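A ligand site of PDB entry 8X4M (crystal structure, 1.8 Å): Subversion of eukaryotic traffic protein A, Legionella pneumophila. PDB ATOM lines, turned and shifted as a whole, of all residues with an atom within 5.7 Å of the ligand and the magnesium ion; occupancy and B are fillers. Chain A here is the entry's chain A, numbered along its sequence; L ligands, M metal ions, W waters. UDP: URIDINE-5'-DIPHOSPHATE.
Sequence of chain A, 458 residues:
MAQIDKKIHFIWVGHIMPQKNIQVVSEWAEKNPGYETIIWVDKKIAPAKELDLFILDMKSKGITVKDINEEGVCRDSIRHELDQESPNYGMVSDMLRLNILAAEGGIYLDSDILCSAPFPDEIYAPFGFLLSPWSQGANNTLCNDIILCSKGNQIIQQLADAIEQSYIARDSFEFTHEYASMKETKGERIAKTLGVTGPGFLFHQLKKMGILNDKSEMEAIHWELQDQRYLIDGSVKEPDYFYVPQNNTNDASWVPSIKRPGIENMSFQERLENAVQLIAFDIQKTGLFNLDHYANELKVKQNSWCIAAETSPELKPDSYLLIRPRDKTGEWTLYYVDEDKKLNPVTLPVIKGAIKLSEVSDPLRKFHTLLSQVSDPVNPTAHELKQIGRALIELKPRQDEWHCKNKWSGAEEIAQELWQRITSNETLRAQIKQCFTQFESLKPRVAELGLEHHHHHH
The nearest printed residue that does not touch the magnesium ion is Asp 145 (4.4 Å).
An oxygen (O2') of the ligand is in hydrogen-bond range of the backbone carbonyl oxygen of Ile 11. O1B of the ligand sits at hydrogen-bond distance from N of Ala 252. N of Ser 253 lies within hydrogen-bond range of O1A of the ligand. OG of Ser 253 sits at hydrogen-bond distance from O1A of the ligand. An oxygen (O1B) of the ligand sits at hydrogen-bond distance from the side-chain amide nitrogen (ND2) of Asn 250 (2.7 Å). The side-chain hydroxyl (OG) of Ser 93 is in hydrogen-bond range of an oxygen (O2') of the ligand (2.8 Å). The backbone NH (N) of Val 13 is in hydrogen-bond range of an oxygen (O2) of the ligand (2.9 Å). O of Val 13 sits at hydrogen-bond distance from N3 of the ligand, at 2.9 Å. The indole nitrogen of Trp 254 sits at hydrogen-bond distance from an oxygen (O3B) of the ligand. The backbone NH of Asp 251 sits at hydrogen-bond distance from an oxygen (O1B) of the ligand (3.5 Å).
Merely in contact with the ligand: Tyr 89, Trp 12, Tyr 108 and Gln 136. Of the 22 residues printed, 14 come within 4 Å of the ligand. The nearest printed residue that does not touch the ligand is Arg 97 (4.2 Å).
Water W6 bridges an oxygen (O3') of the ligand and the backbone NH of Ser 111. Water W4 lies within hydrogen-bond range of O4 of the ligand and N of His 15. Water W2 lies within hydrogen-bond range of OD2 of Asp 251 (2.9 Å) and O1A of the ligand (3.0 Å). Water W5 lies within hydrogen-bond range of O of Leu 109 (2.7 Å), N of Ile 11 (2.9 Å), OH of Tyr 108 (3.0 Å) and O3' of the ligand (3.4 Å).
The magnesium ion is bound by O2B of the ligand (2.0 Å). OD2 of Asp 110 binds the magnesium ion (2.1 Å). Water W3 is bound to the magnesium ion, 2.1 Å away. The magnesium ion is bound by O2A of the ligand (2.1 Å). OD1 of Asp 112 is bound to the magnesium ion. OD2 of Asp 112 is bound to the magnesium ion (2.3 Å). The magnesium ion has six donor atoms within binding distance.
OD1 of Asp 110 is in hydrogen-bond range of OH of Tyr 108 (2.6 Å). The side-chain carboxylate (OD1) of Asp 110 lies within salt-bridge range of the guanidinium group (NH1) of Arg 97 (3.6 Å). The backbone carbonyl oxygen (O) of Asp 145 lies within hydrogen-bond range of the backbone NH (N) of Asp 110. The side-chain carboxylate of Asp 112 sits close to the backbone NH of Asp 251 (2.9 Å). OG of Ser 93 sits at hydrogen-bond distance from NH1 of Arg 97 (2.8 Å). The indole nitrogen (NE1) of Trp 12 lies close to the backbone carbonyl oxygen (O) of His 15, 3.3 Å away. The guanidinium group (NH1) of Arg 97 is in hydrogen-bond range of the side-chain hydroxyl (OH) of Tyr 108 (3.1 Å).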
ATOM      1  N   ILE A  11       8.357 -11.541  27.167  1.00  0.00           N
ATOM      2  CA  ILE A  11       9.620 -12.261  27.014  1.00  0.00           C
ATOM      3  C   ILE A  11      10.725 -11.447  27.684  1.00  0.00           C
ATOM      4  O   ILE A  11      10.832 -10.241  27.481  1.00  0.00           O
ATOM      5  CB  ILE A  11       9.936 -12.519  25.522  1.00  0.00           C
ATOM      6  CG1 ILE A  11       8.877 -13.399  24.850  1.00  0.00           C
ATOM      7  CG2 ILE A  11      11.335 -13.074  25.363  1.00  0.00           C
ATOM      8  CD1 ILE A  11       8.955 -13.390  23.337  1.00  0.00           C
ATOM      9  N   TRP A  12      11.572 -12.132  28.476  1.00  0.00           N
ATOM     10  CA  TRP A  12      12.824 -11.546  28.885  1.00  0.00           C
ATOM     11  C   TRP A  12      13.900 -12.619  29.032  1.00  0.00           C
ATOM     12  O   TRP A  12      13.809 -13.493  29.894  1.00  0.00           O
ATOM     13  CB  TRP A  12      12.690 -10.715  30.168  1.00  0.00           C
ATOM     14  CG  TRP A  12      13.844  -9.778  30.315  1.00  0.00           C
ATOM     15  CD1 TRP A  12      15.071 -10.044  30.846  1.00  0.00           C
ATOM     16  CD2 TRP A  12      13.909  -8.445  29.807  1.00  0.00           C
ATOM     17  NE1 TRP A  12      15.881  -8.952  30.749  1.00  0.00           N
ATOM     18  CE2 TRP A  12      15.198  -7.944  30.111  1.00  0.00           C
ATOM     19  CE3 TRP A  12      13.002  -7.609  29.151  1.00  0.00           C
ATOM     20  CZ2 TRP A  12      15.589  -6.655  29.773  1.00  0.00           C
ATOM     21  CZ3 TRP A  12      13.391  -6.334  28.810  1.00  0.00           C
ATOM     22  CH2 TRP A  12      14.675  -5.863  29.127  1.00  0.00           C
ATOM     23  N   VAL A  13      14.942 -12.490  28.193  1.00  0.00           N
ATOM     24  CA  VAL A  13      16.051 -13.428  28.137  1.00  0.00           C
ATOM     25  C   VAL A  13      17.355 -12.678  28.412  1.00  0.00           C
ATOM     26  O   VAL A  13      17.455 -11.475  28.185  1.00  0.00           O
ATOM     27  CB  VAL A  13      16.083 -14.148  26.775  1.00  0.00           C
ATOM     28  CG1 VAL A  13      14.881 -15.073  26.616  1.00  0.00           C
ATOM     29  CG2 VAL A  13      16.149 -13.171  25.614  1.00  0.00           C
ATOM     30  N   GLY A  14      18.354 -13.419  28.908  1.00  0.00           N
ATOM     31  CA  GLY A  14      19.633 -12.849  29.289  1.00  0.00           C
ATOM     32  C   GLY A  14      19.771 -12.790  30.804  1.00  0.00           C
ATOM     33  O   GLY A  14      19.704 -13.821  31.473  1.00  0.00           O
ATOM     34  N   HIS A  15      19.963 -11.569  31.331  1.00  0.00           N
ATOM     35  CA  HIS A  15      19.935 -11.342  32.762  1.00  0.00           C
ATOM     36  C   HIS A  15      18.483 -11.092  33.172  1.00  0.00           C
ATOM     37  O   HIS A  15      17.565 -11.259  32.370  1.00  0.00           O
ATOM     38  CB  HIS A  15      20.918 -10.237  33.161  1.00  0.00           C
ATOM     39  CG  HIS A  15      21.591 -10.482  34.475  1.00  0.00           C
ATOM     40  ND1 HIS A  15      20.904 -10.688  35.657  1.00  0.00           N
ATOM     41  CD2 HIS A  15      22.894 -10.568  34.790  1.00  0.00           C
ATOM     42  CE1 HIS A  15      21.773 -10.883  36.642  1.00  0.00           C
ATOM     43  NE2 HIS A  15      22.983 -10.818  36.144  1.00  0.00           N
ATOM     44  N   TYR A  89      19.236  -9.634  21.790  1.00  0.00           N
ATOM     45  CA  TYR A  89      18.019 -10.074  22.460  1.00  0.00           C
ATOM     46  C   TYR A  89      16.784  -9.563  21.718  1.00  0.00           C
ATOM     47  O   TYR A  89      15.698 -10.112  21.902  1.00  0.00           O
ATOM     48  CB  TYR A  89      18.023  -9.601  23.913  1.00  0.00           C
ATOM     49  CG  TYR A  89      19.130 -10.171  24.771  1.00  0.00           C
ATOM     50  CD1 TYR A  89      19.296 -11.535  24.904  1.00  0.00           C
ATOM     51  CD2 TYR A  89      19.990  -9.343  25.460  1.00  0.00           C
ATOM     52  CE1 TYR A  89      20.290 -12.062  25.718  1.00  0.00           C
ATOM     53  CE2 TYR A  89      20.996  -9.843  26.272  1.00  0.00           C
ATOM     54  CZ  TYR A  89      21.144 -11.216  26.399  1.00  0.00           C
ATOM     55  OH  TYR A  89      22.141 -11.713  27.201  1.00  0.00           O
ATOM     56  N   GLY A  90      16.949  -8.515  20.915  1.00  0.00           N
ATOM     57  CA  GLY A  90      15.885  -8.045  20.037  1.00  0.00           C
ATOM     58  C   GLY A  90      15.507  -9.118  19.020  1.00  0.00           C
ATOM     59  O   GLY A  90      14.341  -9.454  18.864  1.00  0.00           O
ATOM     60  N   SER A  93      13.919 -12.164  20.790  1.00  0.00           N
ATOM     61  CA  SER A  93      12.556 -11.889  21.209  1.00  0.00           C
ATOM     62  C   SER A  93      11.613 -11.850  20.009  1.00  0.00           C
ATOM     63  O   SER A  93      10.490 -12.339  20.083  1.00  0.00           O
ATOM     64  CB  SER A  93      12.473 -10.604  21.996  1.00  0.00           C
ATOM     65  OG  SER A  93      11.162 -10.388  22.496  1.00  0.00           O
ATOM     66  N   ARG A  97       8.543 -14.668  19.980  1.00  0.00           N
ATOM     67  CA  ARG A  97       7.148 -14.288  20.185  1.00  0.00           C
ATOM     68  C   ARG A  97       6.261 -15.051  19.198  1.00  0.00           C
ATOM     69  O   ARG A  97       5.170 -15.475  19.568  1.00  0.00           O
ATOM     70  CB  ARG A  97       6.939 -12.764  20.100  1.00  0.00           C
ATOM     71  CG  ARG A  97       7.318 -12.120  18.773  1.00  0.00           C
ATOM     72  CD  ARG A  97       7.422 -10.604  18.869  1.00  0.00           C
ATOM     73  NE  ARG A  97       8.537 -10.169  19.714  1.00  0.00           N
ATOM     74  CZ  ARG A  97       8.921  -8.906  19.877  1.00  0.00           C
ATOM     75  NH1 ARG A  97       9.913  -8.611  20.696  1.00  0.00           N
ATOM     76  NH2 ARG A  97       8.291  -7.942  19.228  1.00  0.00           N
ATOM     77  N   TYR A 108       0.958 -11.360  22.571  1.00  0.00           N
ATOM     78  CA  TYR A 108       2.306 -10.943  22.874  1.00  0.00           C
ATOM     79  C   TYR A 108       2.334  -9.420  23.065  1.00  0.00           C
ATOM     80  O   TYR A 108       1.811  -8.696  22.233  1.00  0.00           O
ATOM     81  CB  TYR A 108       3.314 -11.293  21.781  1.00  0.00           C
ATOM     82  CG  TYR A 108       4.632 -10.644  22.078  1.00  0.00           C
ATOM     83  CD1 TYR A 108       5.470 -11.173  23.050  1.00  0.00           C
ATOM     84  CD2 TYR A 108       4.944  -9.392  21.557  1.00  0.00           C
ATOM     85  CE1 TYR A 108       6.643 -10.535  23.409  1.00  0.00           C
ATOM     86  CE2 TYR A 108       6.103  -8.736  21.914  1.00  0.00           C
ATOM     87  CZ  TYR A 108       6.955  -9.305  22.843  1.00  0.00           C
ATOM     88  OH  TYR A 108       8.122  -8.672  23.196  1.00  0.00           O
ATOM     89  N   LEU A 109       2.994  -8.964  24.146  1.00  0.00           N
ATOM     90  CA  LEU A 109       3.264  -7.552  24.383  1.00  0.00           C
ATOM     91  C   LEU A 109       4.719  -7.364  24.810  1.00  0.00           C
ATOM     92  O   LEU A 109       5.242  -8.153  25.585  1.00  0.00           O
ATOM     93  CB  LEU A 109       2.361  -7.031  25.510  1.00  0.00           C
ATOM     94  CG  LEU A 109       0.852  -7.102  25.288  1.00  0.00           C
ATOM     95  CD1 LEU A 109       0.113  -6.677  26.552  1.00  0.00           C
ATOM     96  CD2 LEU A 109       0.428  -6.247  24.101  1.00  0.00           C
ATOM     97  N   ASP A 110       5.348  -6.281  24.332  1.00  0.00           N
ATOM     98  CA  ASP A 110       6.550  -5.762  24.951  1.00  0.00           C
ATOM     99  C   ASP A 110       6.220  -5.278  26.365  1.00  0.00           C
ATOM    100  O   ASP A 110       5.088  -4.900  26.633  1.00  0.00           O
ATOM    101  CB  ASP A 110       7.147  -4.576  24.181  1.00  0.00           C
ATOM    102  CG  ASP A 110       8.027  -4.910  23.000  1.00  0.00           C
ATOM    103  OD1 ASP A 110       8.121  -6.107  22.620  1.00  0.00           O
ATOM    104  OD2 ASP A 110       8.627  -3.958  22.466  1.00  0.00           O
ATOM    105  N   SER A 111       7.240  -5.229  27.234  1.00  0.00           N
ATOM    106  CA  SER A 111       7.077  -4.733  28.597  1.00  0.00           C
ATOM    107  C   SER A 111       7.458  -3.255  28.697  1.00  0.00           C
ATOM    108  O   SER A 111       7.807  -2.792  29.783  1.00  0.00           O
ATOM    109  CB  SER A 111       7.869  -5.573  29.567  1.00  0.00           C
ATOM    110  OG  SER A 111       9.238  -5.610  29.199  1.00  0.00           O
ATOM    111  N   ASP A 112       7.376  -2.512  27.578  1.00  0.00           N
ATOM    112  CA  ASP A 112       7.519  -1.068  27.571  1.00  0.00           C
ATOM    113  C   ASP A 112       6.268  -0.423  26.971  1.00  0.00           C
ATOM    114  O   ASP A 112       6.347   0.641  26.359  1.00  0.00           O
ATOM    115  CB  ASP A 112       8.794  -0.623  26.845  1.00  0.00           C
ATOM    116  CG  ASP A 112       8.930  -1.064  25.399  1.00  0.00           C
ATOM    117  OD1 ASP A 112       8.170  -1.977  24.988  1.00  0.00           O
ATOM    118  OD2 ASP A 112       9.785  -0.497  24.683  1.00  0.00           O
ATOM    119  N   ILE A 113       5.119  -1.088  27.181  1.00  0.00           N
ATOM    120  CA  ILE A 113       3.811  -0.593  26.818  1.00  0.00           C
ATOM    121  C   ILE A 113       2.944  -0.630  28.071  1.00  0.00           C
ATOM    122  O   ILE A 113       2.924  -1.644  28.764  1.00  0.00           O
ATOM    123  CB  ILE A 113       3.171  -1.439  25.693  1.00  0.00           C
ATOM    124  CG1 ILE A 113       4.093  -1.556  24.469  1.00  0.00           C
ATOM    125  CG2 ILE A 113       1.793  -0.915  25.322  1.00  0.00           C
ATOM    126  CD1 ILE A 113       3.646  -2.603  23.461  1.00  0.00           C
ATOM    127  N   GLN A 136       4.351   2.518  19.915  1.00  0.00           N
ATOM    128  CA  GLN A 136       5.301   3.511  20.421  1.00  0.00           C
ATOM    129  C   GLN A 136       4.687   4.909  20.378  1.00  0.00           C
ATOM    130  O   GLN A 136       5.398   5.898  20.172  1.00  0.00           O
ATOM    131  CB  GLN A 136       6.621   3.409  19.646  1.00  0.00           C
ATOM    132  CG  GLN A 136       7.283   2.047  19.820  1.00  0.00           C
ATOM    133  CD  GLN A 136       8.640   1.909  19.184  1.00  0.00           C
ATOM    134  OE1 GLN A 136       9.369   0.951  19.440  1.00  0.00           O
ATOM    135  NE2 GLN A 136       9.000   2.873  18.353  1.00  0.00           N
ATOM    136  N   ASP A 145       5.392  -5.265  18.255  1.00  0.00           N
ATOM    137  CA  ASP A 145       5.474  -5.303  19.711  1.00  0.00           C
ATOM    138  C   ASP A 145       4.117  -5.648  20.318  1.00  0.00           C
ATOM    139  O   ASP A 145       4.007  -5.766  21.539  1.00  0.00           O
ATOM    140  CB  ASP A 145       6.089  -4.026  20.299  1.00  0.00           C
ATOM    141  CG  ASP A 145       5.419  -2.710  19.918  1.00  0.00           C
ATOM    142  OD1 ASP A 145       4.512  -2.741  19.073  1.00  0.00           O
ATOM    143  OD2 ASP A 145       5.828  -1.674  20.481  1.00  0.00           O
ATOM    144  N   ASN A 250       9.504   4.089  24.011  1.00  0.00           N
ATOM    145  CA  ASN A 250      10.013   2.727  23.991  1.00  0.00           C
ATOM    146  C   ASN A 250      11.358   2.707  24.719  1.00  0.00           C
ATOM    147  O   ASN A 250      11.928   3.765  24.992  1.00  0.00           O
ATOM    148  CB  ASN A 250      10.119   2.201  22.562  1.00  0.00           C
ATOM    149  CG  ASN A 250      11.058   3.036  21.709  1.00  0.00           C
ATOM    150  OD1 ASN A 250      10.764   4.204  21.440  1.00  0.00           O
ATOM    151  ND2 ASN A 250      12.172   2.470  21.311  1.00  0.00           N
ATOM    152  N   ASP A 251      11.854   1.499  25.043  1.00  0.00           N
ATOM    153  CA  ASP A 251      13.001   1.341  25.921  1.00  0.00           C
ATOM    154  C   ASP A 251      14.303   1.142  25.131  1.00  0.00           C
ATOM    155  O   ASP A 251      15.366   1.481  25.629  1.00  0.00           O
ATOM    156  CB  ASP A 251      12.802   0.164  26.893  1.00  0.00           C
ATOM    157  CG  ASP A 251      11.982   0.478  28.131  1.00  0.00           C
ATOM    158  OD1 ASP A 251      11.672   1.665  28.366  1.00  0.00           O
ATOM    159  OD2 ASP A 251      11.655  -0.477  28.862  1.00  0.00           O
ATOM    160  N   ALA A 252      14.210   0.569  23.920  1.00  0.00           N
ATOM    161  CA  ALA A 252      15.365   0.235  23.106  1.00  0.00           C
ATOM    162  C   ALA A 252      16.389  -0.566  23.913  1.00  0.00           C
ATOM    163  O   ALA A 252      17.596  -0.354  23.787  1.00  0.00           O
ATOM    164  CB  ALA A 252      15.971   1.503  22.544  1.00  0.00           C
ATOM    165  N   SER A 253      15.900  -1.527  24.701  1.00  0.00           N
ATOM    166  CA  SER A 253      16.703  -2.208  25.703  1.00  0.00           C
ATOM    167  C   SER A 253      17.693  -3.188  25.079  1.00  0.00           C
ATOM    168  O   SER A 253      18.672  -3.575  25.713  1.00  0.00           O
ATOM    169  CB  SER A 253      15.824  -2.891  26.724  1.00  0.00           C
ATOM    170  OG  SER A 253      15.062  -3.928  26.134  1.00  0.00           O
ATOM    171  N   TRP A 254      17.428  -3.598  23.826  1.00  0.00           N
ATOM    172  CA  TRP A 254      18.232  -4.606  23.140  1.00  0.00           C
ATOM    173  C   TRP A 254      19.403  -3.977  22.388  1.00  0.00           C
ATOM    174  O   TRP A 254      20.254  -4.690  21.861  1.00  0.00           O
ATOM    175  CB  TRP A 254      17.359  -5.408  22.157  1.00  0.00           C
ATOM    176  CG  TRP A 254      16.625  -4.540  21.176  1.00  0.00           C
ATOM    177  CD1 TRP A 254      15.410  -3.951  21.362  1.00  0.00           C
ATOM    178  CD2 TRP A 254      17.107  -4.077  19.905  1.00  0.00           C
ATOM    179  NE1 TRP A 254      15.074  -3.193  20.270  1.00  0.00           N
ATOM    180  CE2 TRP A 254      16.095  -3.261  19.358  1.00  0.00           C
ATOM    181  CE3 TRP A 254      18.264  -4.312  19.149  1.00  0.00           C
ATOM    182  CZ2 TRP A 254      16.209  -2.651  18.109  1.00  0.00           C
ATOM    183  CZ3 TRP A 254      18.379  -3.705  17.917  1.00  0.00           C
ATOM    184  CH2 TRP A 254      17.370  -2.894  17.404  1.00  0.00           C
HETATM  185  N1  UDP L   1      14.992  -8.179  25.508  1.00  0.00           N
HETATM  186  C2  UDP L   1      15.431  -9.235  26.278  1.00  0.00           C
HETATM  187  N3  UDP L   1      16.540  -8.974  27.036  1.00  0.00           N
HETATM  188  C4  UDP L   1      17.260  -7.794  27.090  1.00  0.00           C
HETATM  189  C5  UDP L   1      16.750  -6.751  26.252  1.00  0.00           C
HETATM  190  C6  UDP L   1      15.656  -6.971  25.495  1.00  0.00           C
HETATM  191  O2  UDP L   1      14.865 -10.318  26.306  1.00  0.00           O
HETATM  192  O4  UDP L   1      18.238  -7.715  27.815  1.00  0.00           O
HETATM  193  C1' UDP L   1      13.805  -8.413  24.672  1.00  0.00           C
HETATM  194  C2' UDP L   1      12.510  -8.401  25.483  1.00  0.00           C
HETATM  195  O2' UDP L   1      11.716  -9.490  25.074  1.00  0.00           O
HETATM  196  C3' UDP L   1      11.896  -7.052  25.103  1.00  0.00           C
HETATM  197  C4' UDP L   1      12.340  -6.932  23.642  1.00  0.00           C
HETATM  198  O4' UDP L   1      13.703  -7.402  23.682  1.00  0.00           O
HETATM  199  O3' UDP L   1      10.476  -7.027  25.226  1.00  0.00           O
HETATM  200  C5' UDP L   1      12.253  -5.553  23.030  1.00  0.00           C
HETATM  201  O5' UDP L   1      12.918  -4.613  23.899  1.00  0.00           O
HETATM  202  PA  UDP L   1      12.384  -3.101  23.958  1.00  0.00           P
HETATM  203  O1A UDP L   1      13.197  -2.362  24.952  1.00  0.00           O
HETATM  204  O2A UDP L   1      10.913  -3.119  24.147  1.00  0.00           O
HETATM  205  O3A UDP L   1      12.726  -2.588  22.488  1.00  0.00           O
HETATM  206  PB  UDP L   1      12.036  -1.487  21.544  1.00  0.00           P
HETATM  207  O1B UDP L   1      12.454  -0.143  22.034  1.00  0.00           O
HETATM  208  O2B UDP L   1      10.560  -1.702  21.648  1.00  0.00           O
HETATM  209  O3B UDP L   1      12.552  -1.773  20.179  1.00  0.00           O
HETATM  210 MG    MG M   1       9.347  -2.130  23.123  1.00  0.00          MG
HETATM  211  O   HOH W   1      20.662  -6.272  27.410  1.00  0.00           O
HETATM  212  O   HOH W   2      11.954  -3.048  27.566  1.00  0.00           O
HETATM  213  O   HOH W   3       7.793  -1.069  22.233  1.00  0.00           O
HETATM  214  O   HOH W   4      19.579  -9.049  29.924  1.00  0.00           O
HETATM  215  O   HOH W   5       7.797  -8.872  26.144  1.00  0.00           O
HETATM  216  O   HOH W   6      10.058  -4.525  26.324  1.00  0.00           O
